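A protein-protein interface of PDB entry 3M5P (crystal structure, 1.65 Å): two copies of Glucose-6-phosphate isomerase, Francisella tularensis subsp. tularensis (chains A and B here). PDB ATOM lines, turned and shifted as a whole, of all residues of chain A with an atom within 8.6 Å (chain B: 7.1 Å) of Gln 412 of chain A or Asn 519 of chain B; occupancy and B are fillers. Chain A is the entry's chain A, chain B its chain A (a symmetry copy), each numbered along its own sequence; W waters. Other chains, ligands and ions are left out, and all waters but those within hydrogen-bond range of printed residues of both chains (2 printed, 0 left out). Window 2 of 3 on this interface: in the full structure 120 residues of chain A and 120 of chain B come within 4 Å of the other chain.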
ATOM      1  N   THR A 376       1.553  33.644  10.413  1.00  0.00           N
ATOM      2  CA  THR A 376       2.458  32.517  10.600  1.00  0.00           C
ATOM      3  C   THR A 376       3.779  32.856  11.257  1.00  0.00           C
ATOM      4  O   THR A 376       4.573  31.960  11.517  1.00  0.00           O
ATOM      5  CB  THR A 376       2.777  31.825   9.224  1.00  0.00           C
ATOM      6  OG1 THR A 376       3.586  32.711   8.436  1.00  0.00           O
ATOM      7  CG2 THR A 376       1.459  31.446   8.444  1.00  0.00           C
ATOM      8  N   ILE A 400      -9.107  33.551  10.236  1.00  0.00           N
ATOM      9  CA  ILE A 400     -10.050  34.384   9.503  1.00  0.00           C
ATOM     10  C   ILE A 400     -10.221  33.813   8.082  1.00  0.00           C
ATOM     11  O   ILE A 400      -9.253  33.692   7.333  1.00  0.00           O
ATOM     12  CB  ILE A 400      -9.562  35.842   9.399  1.00  0.00           C
ATOM     13  CG1 ILE A 400      -9.028  36.374  10.767  1.00  0.00           C
ATOM     14  CG2 ILE A 400     -10.686  36.739   8.808  1.00  0.00           C
ATOM     15  CD1 ILE A 400     -10.047  36.485  11.909  1.00  0.00           C
ATOM     16  N   ALA A 401     -11.430  33.367   7.737  1.00  0.00           N
ATOM     17  CA  ALA A 401     -11.606  32.616   6.502  1.00  0.00           C
ATOM     18  C   ALA A 401     -11.253  33.445   5.244  1.00  0.00           C
ATOM     19  O   ALA A 401     -10.632  32.942   4.295  1.00  0.00           O
ATOM     20  CB  ALA A 401     -13.030  32.057   6.422  1.00  0.00           C
ATOM     21  N   THR A 402     -11.683  34.698   5.209  1.00  0.00           N
ATOM     22  CA  THR A 402     -11.467  35.557   4.067  1.00  0.00           C
ATOM     23  C   THR A 402     -10.917  36.866   4.560  1.00  0.00           C
ATOM     24  O   THR A 402     -11.296  37.362   5.633  1.00  0.00           O
ATOM     25  CB  THR A 402     -12.787  35.803   3.255  1.00  0.00           C
ATOM     26  OG1 THR A 402     -13.710  36.493   4.091  1.00  0.00           O
ATOM     27  CG2 THR A 402     -13.405  34.513   2.822  1.00  0.00           C
ATOM     28  N   SER A 403      -9.991  37.408   3.788  1.00  0.00           N
ATOM     29  CA  SER A 403      -9.314  38.630   4.113  1.00  0.00           C
ATOM     30  C   SER A 403      -9.877  39.758   3.266  1.00  0.00           C
ATOM     31  O   SER A 403     -11.036  39.689   2.828  1.00  0.00           O
ATOM     32  CB  SER A 403      -7.809  38.452   3.870  1.00  0.00           C
ATOM     33  OG  SER A 403      -7.092  39.605   4.246  1.00  0.00           O
ATOM     34  N   HIS A 405      -8.322  41.276   0.521  1.00  0.00           N
ATOM     35  CA  HIS A 405      -7.606  41.383  -0.763  1.00  0.00           C
ATOM     36  C   HIS A 405      -7.861  40.140  -1.584  1.00  0.00           C
ATOM     37  O   HIS A 405      -8.501  39.191  -1.109  1.00  0.00           O
ATOM     38  CB  HIS A 405      -6.102  41.499  -0.473  1.00  0.00           C
ATOM     39  CG  HIS A 405      -5.593  40.328   0.283  1.00  0.00           C
ATOM     40  ND1 HIS A 405      -5.381  39.109  -0.320  1.00  0.00           N
ATOM     41  CD2 HIS A 405      -5.385  40.141   1.603  1.00  0.00           C
ATOM     42  CE1 HIS A 405      -5.030  38.228   0.600  1.00  0.00           C
ATOM     43  NE2 HIS A 405      -5.041  38.829   1.777  1.00  0.00           N
ATOM     44  N   TYR A 407      -5.320  38.184  -3.075  1.00  0.00           N
ATOM     45  CA  TYR A 407      -4.197  37.216  -3.090  1.00  0.00           C
ATOM     46  C   TYR A 407      -4.634  35.899  -2.459  1.00  0.00           C
ATOM     47  O   TYR A 407      -4.204  35.534  -1.357  1.00  0.00           O
ATOM     48  CB  TYR A 407      -2.946  37.770  -2.382  1.00  0.00           C
ATOM     49  CG  TYR A 407      -2.247  38.852  -3.155  1.00  0.00           C
ATOM     50  CD1 TYR A 407      -1.164  38.545  -3.964  1.00  0.00           C
ATOM     51  CD2 TYR A 407      -2.676  40.165  -3.110  1.00  0.00           C
ATOM     52  CE1 TYR A 407      -0.507  39.500  -4.677  1.00  0.00           C
ATOM     53  CE2 TYR A 407      -2.020  41.150  -3.867  1.00  0.00           C
ATOM     54  CZ  TYR A 407      -0.927  40.799  -4.620  1.00  0.00           C
ATOM     55  OH  TYR A 407      -0.259  41.740  -5.344  1.00  0.00           O
ATOM     56  N   ASP A 408      -5.479  35.167  -3.188  1.00  0.00           N
ATOM     57  CA  ASP A 408      -6.124  33.979  -2.657  1.00  0.00           C
ATOM     58  C   ASP A 408      -5.115  32.880  -2.294  1.00  0.00           C
ATOM     59  O   ASP A 408      -5.344  32.096  -1.348  1.00  0.00           O
ATOM     60  CB  ASP A 408      -7.117  33.428  -3.657  1.00  0.00           C
ATOM     61  CG  ASP A 408      -8.295  34.356  -3.860  1.00  0.00           C
ATOM     62  OD1 ASP A 408      -8.484  35.325  -3.085  1.00  0.00           O
ATOM     63  OD2 ASP A 408      -9.048  34.070  -4.782  1.00  0.00           O
ATOM     64  N   ASN A 409      -4.036  32.796  -3.072  1.00  0.00           N
ATOM     65  CA  ASN A 409      -2.969  31.852  -2.754  1.00  0.00           C
ATOM     66  C   ASN A 409      -2.304  32.133  -1.388  1.00  0.00           C
ATOM     67  O   ASN A 409      -2.028  31.198  -0.646  1.00  0.00           O
ATOM     68  CB  ASN A 409      -1.935  31.800  -3.880  1.00  0.00           C
ATOM     69  CG  ASN A 409      -1.226  33.106  -4.130  1.00  0.00           C
ATOM     70  OD1 ASN A 409      -1.743  34.206  -3.918  1.00  0.00           O
ATOM     71  ND2 ASN A 409      -0.029  32.980  -4.677  1.00  0.00           N
ATOM     72  N   HIS A 410      -2.116  33.405  -1.040  1.00  0.00           N
ATOM     73  CA  HIS A 410      -1.577  33.783   0.255  1.00  0.00           C
ATOM     74  C   HIS A 410      -2.543  33.426   1.386  1.00  0.00           C
ATOM     75  O   HIS A 410      -2.174  32.856   2.438  1.00  0.00           O
ATOM     76  CB  HIS A 410      -1.285  35.290   0.331  1.00  0.00           C
ATOM     77  CG  HIS A 410      -0.066  35.725  -0.414  1.00  0.00           C
ATOM     78  ND1 HIS A 410       1.067  36.178   0.243  1.00  0.00           N
ATOM     79  CD2 HIS A 410       0.219  35.774  -1.744  1.00  0.00           C
ATOM     80  CE1 HIS A 410       1.981  36.515  -0.650  1.00  0.00           C
ATOM     81  NE2 HIS A 410       1.508  36.264  -1.860  1.00  0.00           N
ATOM     82  N   GLN A 411      -3.811  33.760   1.165  1.00  0.00           N
ATOM     83  CA  GLN A 411      -4.834  33.471   2.158  1.00  0.00           C
ATOM     84  C   GLN A 411      -4.975  31.952   2.396  1.00  0.00           C
ATOM     85  O   GLN A 411      -5.097  31.515   3.529  1.00  0.00           O
ATOM     86  CB  GLN A 411      -6.163  34.131   1.773  1.00  0.00           C
ATOM     87  CG  GLN A 411      -7.252  33.869   2.781  1.00  0.00           C
ATOM     88  CD  GLN A 411      -7.060  34.600   4.111  1.00  0.00           C
ATOM     89  OE1 GLN A 411      -6.154  35.437   4.260  1.00  0.00           O
ATOM     90  NE2 GLN A 411      -7.932  34.313   5.072  1.00  0.00           N
ATOM     91  N   GLN A 412      -4.931  31.151   1.338  1.00  0.00           N
ATOM     92  CA  GLN A 412      -5.026  29.710   1.450  1.00  0.00           C
ATOM     93  C   GLN A 412      -3.811  29.145   2.219  1.00  0.00           C
ATOM     94  O   GLN A 412      -3.977  28.315   3.082  1.00  0.00           O
ATOM     95  CB  GLN A 412      -5.139  29.075   0.070  1.00  0.00           C
ATOM     96  CG  GLN A 412      -5.411  27.608   0.129  1.00  0.00           C
ATOM     97  CD  GLN A 412      -5.359  26.951  -1.234  1.00  0.00           C
ATOM     98  OE1 GLN A 412      -6.345  26.416  -1.674  1.00  0.00           O
ATOM     99  NE2 GLN A 412      -4.217  27.027  -1.912  1.00  0.00           N
ATOM    100  N   ALA A 413      -2.601  29.622   1.907  1.00  0.00           N
ATOM    101  CA  ALA A 413      -1.408  29.226   2.632  1.00  0.00           C
ATOM    102  C   ALA A 413      -1.476  29.626   4.123  1.00  0.00           C
ATOM    103  O   ALA A 413      -1.094  28.853   4.985  1.00  0.00           O
ATOM    104  CB  ALA A 413      -0.153  29.837   1.949  1.00  0.00           C
ATOM    105  N   LEU A 414      -1.978  30.829   4.422  1.00  0.00           N
ATOM    106  CA  LEU A 414      -2.119  31.285   5.802  1.00  0.00           C
ATOM    107  C   LEU A 414      -2.996  30.316   6.606  1.00  0.00           C
ATOM    108  O   LEU A 414      -2.621  29.860   7.680  1.00  0.00           O
ATOM    109  CB  LEU A 414      -2.703  32.685   5.803  1.00  0.00           C
ATOM    110  CG  LEU A 414      -2.994  33.353   7.150  1.00  0.00           C
ATOM    111  CD1 LEU A 414      -1.700  33.527   8.020  1.00  0.00           C
ATOM    112  CD2 LEU A 414      -3.809  34.679   6.897  1.00  0.00           C
ATOM    113  N   LEU A 415      -4.146  29.966   6.056  1.00  0.00           N
ATOM    114  CA  LEU A 415      -5.043  29.055   6.722  1.00  0.00           C
ATOM    115  C   LEU A 415      -4.469  27.648   6.794  1.00  0.00           C
ATOM    116  O   LEU A 415      -4.631  26.983   7.810  1.00  0.00           O
ATOM    117  CB  LEU A 415      -6.389  29.042   5.987  1.00  0.00           C
ATOM    118  CG  LEU A 415      -7.218  30.322   6.124  1.00  0.00           C
ATOM    119  CD1 LEU A 415      -8.287  30.364   4.975  1.00  0.00           C
ATOM    120  CD2 LEU A 415      -7.791  30.495   7.556  1.00  0.00           C
ATOM    121  N   ALA A 416      -3.873  27.155   5.707  1.00  0.00           N
ATOM    122  CA  ALA A 416      -3.250  25.823   5.736  1.00  0.00           C
ATOM    123  C   ALA A 416      -2.239  25.708   6.865  1.00  0.00           C
ATOM    124  O   ALA A 416      -2.183  24.691   7.569  1.00  0.00           O
ATOM    125  CB  ALA A 416      -2.609  25.438   4.353  1.00  0.00           C
ATOM    126  N   ASN A 417      -1.455  26.770   7.054  1.00  0.00           N
ATOM    127  CA  ASN A 417      -0.476  26.817   8.146  1.00  0.00           C
ATOM    128  C   ASN A 417      -1.155  26.816   9.516  1.00  0.00           C
ATOM    129  O   ASN A 417      -0.758  26.077  10.422  1.00  0.00           O
ATOM    130  CB  ASN A 417       0.462  28.002   8.004  1.00  0.00           C
ATOM    131  CG  ASN A 417       1.627  27.708   7.092  1.00  0.00           C
ATOM    132  OD1 ASN A 417       2.614  27.100   7.533  1.00  0.00           O
ATOM    133  ND2 ASN A 417       1.512  28.070   5.813  1.00  0.00           N
ATOM    134  N   CYS A 418      -2.216  27.593   9.666  1.00  0.00           N
ATOM    135  CA  CYS A 418      -2.931  27.615  10.931  1.00  0.00           C
ATOM    136  C   CYS A 418      -3.406  26.231  11.294  1.00  0.00           C
ATOM    137  O   CYS A 418      -3.174  25.746  12.400  1.00  0.00           O
ATOM    138  CB  CYS A 418      -4.129  28.567  10.835  1.00  0.00           C
ATOM    139  SG  CYS A 418      -5.066  28.755  12.350  1.00  0.00           S
ATOM    140  N   PHE A 419      -4.064  25.573  10.342  1.00  0.00           N
ATOM    141  CA  PHE A 419      -4.643  24.251  10.596  1.00  0.00           C
ATOM    142  C   PHE A 419      -3.559  23.164  10.756  1.00  0.00           C
ATOM    143  O   PHE A 419      -3.710  22.243  11.546  1.00  0.00           O
ATOM    144  CB  PHE A 419      -5.628  23.872   9.479  1.00  0.00           C
ATOM    145  CG  PHE A 419      -6.757  24.866   9.258  1.00  0.00           C
ATOM    146  CD1 PHE A 419      -7.138  25.758  10.239  1.00  0.00           C
ATOM    147  CD2 PHE A 419      -7.405  24.917   8.035  1.00  0.00           C
ATOM    148  CE1 PHE A 419      -8.180  26.640  10.022  1.00  0.00           C
ATOM    149  CE2 PHE A 419      -8.441  25.822   7.833  1.00  0.00           C
ATOM    150  CZ  PHE A 419      -8.812  26.674   8.822  1.00  0.00           C
ATOM    151  N   VAL B 178       3.014  35.308   5.506  1.00  0.00           N
ATOM    152  CA  VAL B 178       2.380  34.945   4.240  1.00  0.00           C
ATOM    153  C   VAL B 178       1.021  35.683   4.072  1.00  0.00           C
ATOM    154  O   VAL B 178       0.578  35.907   2.969  1.00  0.00           O
ATOM    155  CB  VAL B 178       2.217  33.420   4.030  1.00  0.00           C
ATOM    156  CG1 VAL B 178       1.227  32.757   5.004  1.00  0.00           C
ATOM    157  CG2 VAL B 178       1.870  33.070   2.538  1.00  0.00           C
ATOM    158  N   GLU B 207       8.357  28.691   2.781  1.00  0.00           N
ATOM    159  CA  GLU B 207       7.133  28.908   2.029  1.00  0.00           C
ATOM    160  C   GLU B 207       6.690  30.346   1.985  1.00  0.00           C
ATOM    161  O   GLU B 207       6.384  30.869   0.913  1.00  0.00           O
ATOM    162  CB  GLU B 207       5.999  28.083   2.650  1.00  0.00           C
ATOM    163  CG  GLU B 207       4.669  28.238   1.887  1.00  0.00           C
ATOM    164  CD  GLU B 207       3.456  27.762   2.638  1.00  0.00           C
ATOM    165  OE1 GLU B 207       3.476  27.710   3.881  1.00  0.00           O
ATOM    166  OE2 GLU B 207       2.454  27.480   1.962  1.00  0.00           O
ATOM    167  N   LEU B 211       6.588  32.766  -1.378  1.00  0.00           N
ATOM    168  CA  LEU B 211       5.307  33.296  -1.893  1.00  0.00           C
ATOM    169  C   LEU B 211       5.362  34.817  -1.944  1.00  0.00           C
ATOM    170  O   LEU B 211       4.960  35.428  -2.938  1.00  0.00           O
ATOM    171  CB  LEU B 211       4.083  32.879  -1.057  1.00  0.00           C
ATOM    172  CG  LEU B 211       3.251  31.681  -1.514  1.00  0.00           C
ATOM    173  CD1 LEU B 211       4.135  30.536  -1.764  1.00  0.00           C
ATOM    174  CD2 LEU B 211       2.188  31.307  -0.504  1.00  0.00           C
ATOM    175  N   GLY B 511       1.385  21.272   6.477  1.00  0.00           N
ATOM    176  CA  GLY B 511       0.850  22.418   5.720  1.00  0.00           C
ATOM    177  C   GLY B 511       0.772  22.089   4.247  1.00  0.00           C
ATOM    178  O   GLY B 511      -0.205  22.405   3.582  1.00  0.00           O
ATOM    179  N   ASN B 513       0.395  19.056   2.946  1.00  0.00           N
ATOM    180  CA  ASN B 513      -0.664  18.065   2.794  1.00  0.00           C
ATOM    181  C   ASN B 513      -2.038  18.747   2.877  1.00  0.00           C
ATOM    182  O   ASN B 513      -2.942  18.384   2.171  1.00  0.00           O
ATOM    183  CB  ASN B 513      -0.652  17.016   3.911  1.00  0.00           C
ATOM    184  CG  ASN B 513       0.590  16.145   3.932  1.00  0.00           C
ATOM    185  OD1 ASN B 513       1.282  15.971   2.929  1.00  0.00           O
ATOM    186  ND2 ASN B 513       0.862  15.555   5.115  1.00  0.00           N
ATOM    187  N   ILE B 514      -2.189  19.698   3.803  1.00  0.00           N
ATOM    188  CA  ILE B 514      -3.448  20.418   3.951  1.00  0.00           C
ATOM    189  C   ILE B 514      -3.761  21.268   2.705  1.00  0.00           C
ATOM    190  O   ILE B 514      -4.914  21.324   2.266  1.00  0.00           O
ATOM    191  CB  ILE B 514      -3.461  21.232   5.269  1.00  0.00           C
ATOM    192  CG1 ILE B 514      -3.598  20.224   6.442  1.00  0.00           C
ATOM    193  CG2 ILE B 514      -4.594  22.293   5.308  1.00  0.00           C
ATOM    194  CD1 ILE B 514      -3.323  20.820   7.836  1.00  0.00           C
ATOM    195  N   LEU B 515      -2.739  21.874   2.103  1.00  0.00           N
ATOM    196  CA  LEU B 515      -2.958  22.632   0.879  1.00  0.00           C
ATOM    197  C   LEU B 515      -3.474  21.714  -0.210  1.00  0.00           C
ATOM    198  O   LEU B 515      -4.395  22.082  -0.920  1.00  0.00           O
ATOM    199  CB  LEU B 515      -1.692  23.316   0.391  1.00  0.00           C
ATOM    200  CG  LEU B 515      -1.332  24.665   0.935  1.00  0.00           C
ATOM    201  CD1 LEU B 515       0.037  25.062   0.320  1.00  0.00           C
ATOM    202  CD2 LEU B 515      -2.440  25.729   0.651  1.00  0.00           C
ATOM    203  N   LYS B 516      -2.885  20.524  -0.332  1.00  0.00           N
ATOM    204  CA  LYS B 516      -3.387  19.529  -1.280  1.00  0.00           C
ATOM    205  C   LYS B 516      -4.853  19.152  -0.991  1.00  0.00           C
ATOM    206  O   LYS B 516      -5.642  19.036  -1.917  1.00  0.00           O
ATOM    207  CB  LYS B 516      -2.522  18.265  -1.284  1.00  0.00           C
ATOM    208  CG  LYS B 516      -1.229  18.446  -2.026  1.00  0.00           C
ATOM    209  CD  LYS B 516      -0.315  17.229  -1.907  1.00  0.00           C
ATOM    210  CE  LYS B 516       1.058  17.508  -2.529  1.00  0.00           C
ATOM    211  NZ  LYS B 516       1.205  16.777  -3.833  1.00  0.00           N
ATOM    212  N   ALA B 517      -5.189  18.947   0.281  1.00  0.00           N
ATOM    213  CA  ALA B 517      -6.533  18.584   0.699  1.00  0.00           C
ATOM    214  C   ALA B 517      -7.527  19.706   0.403  1.00  0.00           C
ATOM    215  O   ALA B 517      -8.649  19.440  -0.027  1.00  0.00           O
ATOM    216  CB  ALA B 517      -6.558  18.199   2.179  1.00  0.00           C
ATOM    217  N   MET B 518      -7.122  20.950   0.653  1.00  0.00           N
ATOM    218  CA  MET B 518      -7.930  22.131   0.327  1.00  0.00           C
ATOM    219  C   MET B 518      -8.225  22.288  -1.171  1.00  0.00           C
ATOM    220  O   MET B 518      -9.224  22.889  -1.543  1.00  0.00           O
ATOM    221  CB  MET B 518      -7.252  23.400   0.842  1.00  0.00           C
ATOM    222  CG  MET B 518      -7.252  23.510   2.338  1.00  0.00           C
ATOM    223  SD  MET B 518      -6.309  25.054   3.039  1.00  0.00           S
ATOM    224  CE  MET B 518      -7.708  26.430   2.840  1.00  0.00           C
ATOM    225  N   ASN B 519      -7.338  21.802  -2.023  1.00  0.00           N
ATOM    226  CA  ASN B 519      -7.530  21.920  -3.482  1.00  0.00           C
ATOM    227  C   ASN B 519      -8.216  20.736  -4.127  1.00  0.00           C
ATOM    228  O   ASN B 519      -8.638  20.831  -5.281  1.00  0.00           O
ATOM    229  CB  ASN B 519      -6.191  22.206  -4.168  1.00  0.00           C
ATOM    230  CG  ASN B 519      -5.695  23.618  -3.872  1.00  0.00           C
ATOM    231  OD1 ASN B 519      -6.463  24.580  -3.962  1.00  0.00           O
ATOM    232  ND2 ASN B 519      -4.420  23.749  -3.502  1.00  0.00           N
ATOM    233  N   ASP B 520      -8.342  19.632  -3.392  1.00  0.00           N
ATOM    234  CA  ASP B 520      -8.883  18.406  -3.975  1.00  0.00           C
ATOM    235  C   ASP B 520      -9.371  17.465  -2.868  1.00  0.00           C
ATOM    236  O   ASP B 520      -8.594  16.694  -2.293  1.00  0.00           O
ATOM    237  CB  ASP B 520      -7.806  17.748  -4.841  1.00  0.00           C
ATOM    238  CG  ASP B 520      -8.299  16.511  -5.573  1.00  0.00           C
ATOM    239  OD1 ASP B 520      -7.448  15.811  -6.170  1.00  0.00           O
ATOM    240  OD2 ASP B 520      -9.519  16.230  -5.561  1.00  0.00           O
ATOM    241  N   ASP B 521     -10.669  17.528  -2.601  1.00  0.00           N
ATOM    242  CA  ASP B 521     -11.293  16.692  -1.582  1.00  0.00           C
ATOM    243  C   ASP B 521     -11.405  15.206  -1.934  1.00  0.00           C
ATOM    244  O   ASP B 521     -11.862  14.418  -1.100  1.00  0.00           O
ATOM    245  CB  ASP B 521     -12.669  17.255  -1.213  1.00  0.00           C
ATOM    246  CG  ASP B 521     -13.645  17.287  -2.389  1.00  0.00           C
ATOM    247  OD1 ASP B 521     -13.433  16.583  -3.402  1.00  0.00           O
ATOM    248  OD2 ASP B 521     -14.637  18.040  -2.287  1.00  0.00           O
ATOM    249  N   SER B 522     -11.018  14.834  -3.160  1.00  0.00           N
ATOM    250  CA  SER B 522     -10.909  13.439  -3.553  1.00  0.00           C
ATOM    251  C   SER B 522      -9.476  12.919  -3.380  1.00  0.00           C
ATOM    252  O   SER B 522      -9.170  11.803  -3.795  1.00  0.00           O
ATOM    253  CB  SER B 522     -11.365  13.251  -5.016  1.00  0.00           C
ATOM    254  OG  SER B 522     -10.289  13.440  -5.931  1.00  0.00           O
ATOM    255  N   SER B 523      -8.600  13.715  -2.774  1.00  0.00           N
ATOM    256  CA  SER B 523      -7.209  13.316  -2.619  1.00  0.00           C
ATOM    257  C   SER B 523      -7.034  12.372  -1.430  1.00  0.00           C
ATOM    258  O   SER B 523      -7.844  12.362  -0.491  1.00  0.00           O
ATOM    259  CB  SER B 523      -6.314  14.550  -2.429  1.00  0.00           C
ATOM    260  OG  SER B 523      -6.696  15.303  -1.284  1.00  0.00           O
ATOM    261  N   TYR B 526      -6.835  14.514   1.723  1.00  0.00           N
ATOM    262  CA  TYR B 526      -8.110  14.875   2.327  1.00  0.00           C
ATOM    263  C   TYR B 526      -8.735  13.700   3.128  1.00  0.00           C
ATOM    264  O   TYR B 526      -9.186  13.865   4.285  1.00  0.00           O
ATOM    265  CB  TYR B 526      -9.069  15.387   1.239  1.00  0.00           C
ATOM    266  CG  TYR B 526     -10.366  15.922   1.774  1.00  0.00           C
ATOM    267  CD1 TYR B 526     -10.564  17.283   1.955  1.00  0.00           C
ATOM    268  CD2 TYR B 526     -11.410  15.065   2.098  1.00  0.00           C
ATOM    269  CE1 TYR B 526     -11.768  17.780   2.445  1.00  0.00           C
ATOM    270  CE2 TYR B 526     -12.619  15.557   2.600  1.00  0.00           C
ATOM    271  CZ  TYR B 526     -12.796  16.897   2.751  1.00  0.00           C
ATOM    272  OH  TYR B 526     -13.982  17.367   3.257  1.00  0.00           O
ATOM    273  N   ILE B 537     -11.408  23.048   7.079  1.00  0.00           N
ATOM    274  CA  ILE B 537     -11.279  23.269   5.643  1.00  0.00           C
ATOM    275  C   ILE B 537     -12.683  23.438   5.015  1.00  0.00           C
ATOM    276  O   ILE B 537     -12.888  24.326   4.194  1.00  0.00           O
ATOM    277  CB  ILE B 537     -10.515  22.104   4.977  1.00  0.00           C
ATOM    278  CG1 ILE B 537      -9.033  22.136   5.332  1.00  0.00           C
ATOM    279  CG2 ILE B 537     -10.697  22.091   3.475  1.00  0.00           C
ATOM    280  CD1 ILE B 537      -8.300  20.872   4.835  1.00  0.00           C
ATOM    281  N   VAL B 540     -14.181  26.938   5.745  1.00  0.00           N
ATOM    282  CA  VAL B 540     -13.584  27.982   4.931  1.00  0.00           C
ATOM    283  C   VAL B 540     -14.149  28.011   3.519  1.00  0.00           C
ATOM    284  O   VAL B 540     -14.434  29.090   2.999  1.00  0.00           O
ATOM    285  CB  VAL B 540     -12.051  27.857   4.898  1.00  0.00           C
ATOM    286  CG1 VAL B 540     -11.491  28.792   3.885  1.00  0.00           C
ATOM    287  CG2 VAL B 540     -11.494  28.123   6.312  1.00  0.00           C
ATOM    288  N   LYS B 541     -14.339  26.830   2.943  1.00  0.00           N
ATOM    289  CA  LYS B 541     -14.885  26.649   1.592  1.00  0.00           C
ATOM    290  C   LYS B 541     -16.325  27.117   1.418  1.00  0.00           C
ATOM    291  O   LYS B 541     -16.732  27.410   0.285  1.00  0.00           O
ATOM    292  CB  LYS B 541     -14.852  25.164   1.215  1.00  0.00           C
ATOM    293  CG  LYS B 541     -13.478  24.566   1.123  1.00  0.00           C
ATOM    294  CD  LYS B 541     -13.014  24.445  -0.332  1.00  0.00           C
ATOM    295  CE  LYS B 541     -11.515  24.181  -0.395  1.00  0.00           C
ATOM    296  NZ  LYS B 541     -10.754  25.198   0.412  1.00  0.00           N
HETATM  297  O   HOH W   1       3.077  33.995  -4.692  1.00  0.00           O
HETATM  298  O   HOH W   2       4.727  26.248   6.148  1.00  0.00           O
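Water W2 lies within hydrogen-bond range of OD1 of Asn 417 of chain A and OE1 of Glu 207 of chain B.
Water W1 bridges O of Leu 211 of chain B (2.9 Å) and ND2 of Asn 409 of chain A (3.3 Å).
A ring nitrogen (ND1) of His 410 of chain A lies within hydrogen-bond range of the backbone carbonyl oxygen of Val 178 of chain B (2.8 Å).
OE1 of Gln 412 of chain A sits close to OD1 of Asn 519 of chain B, 2.9 Å away.
The side-chain amide nitrogen of Asn 417 of chain A is in hydrogen-bond range of the side-chain carboxylate of Glu 207 of chain B, 2.8 Å away.
Of the 19 printed residues of chain A, 9 touch a printed residue of chain B.
Hydrophobic or aromatic side chains of chain A that line the printed part of chain B: His 410, Ala 413, Leu 415, Ala 416 and Phe 419.
Among the printed residues, 18 pairs touch across the chains.
Gln 412 of chain A touches three residues of chain B.
Asn 519 of chain B touches just one residue of chain A: Gln 412.
Of the printed residues of chain A, Gly 511 of chain B touches Ala 416 (3.9 Å).
Of the printed residues of chain B, Leu 415 of chain A touches Val 540 (3.7 Å).
Of the printed residues of chain A, Leu 515 of chain B touches Gln 412 (3.4 Å) and Ala 416 (3.7 Å).
Ser 523 of chain B touches none of the printed residues of chain A.
The nearest residue of chain B that does not touch Gln 412 of chain A is Lys 541 of chain B (5.0 Å).
The nearest printed residue of chain A that does not touch Glu 207 of chain B is Ala 416 of chain A (6.0 Å).
O of Ala 413 of chain A lies within hydrogen-bond range of ND2 of Asn 417 of chain A, at 2.8 Å.
The side-chain amide nitrogen of Asn 519 of chain B sits at hydrogen-bond distance from the backbone carbonyl oxygen of Leu 515 of chain B (3.1 Å).
The backbone carbonyl oxygen of Met 518 of chain B sits close to the side-chain amino group of Lys 541 of chain B, 3.4 Å away.
Thr 376 of chain A touches Val 178 of chain B.
His 410 of chain A touches Leu 211 of chain B.
Val 178 of chain B touches Ala 413 of chain A (CG2 to CB, 3.9 Å).
CB of Ala 413 of chain A touches OE2 of Glu 207 of chain B (3.5 Å).
Val 178 of chain B touches Leu 414 of chain A.
Leu 415 of chain A touches Val 540 of chain B (CD1 to CG1, 3.7 Å).
Gly 511 of chain B touches Ala 416 of chain A (O to CB, 3.9 Å).
Met 518 of chain B touches Ala 416 of chain A (SD to CB, 3.9 Å).
C of Phe 419 of chain A touches CD1 of Ile 514 of chain B, 3.8 Å away.
Phe 419 of chain A touches Val 540 of chain B.
No position is printed for both chains.
Of the 18 pairs that touch across the chains among the printed residues, none has its exchanged pair printed and touching as well.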
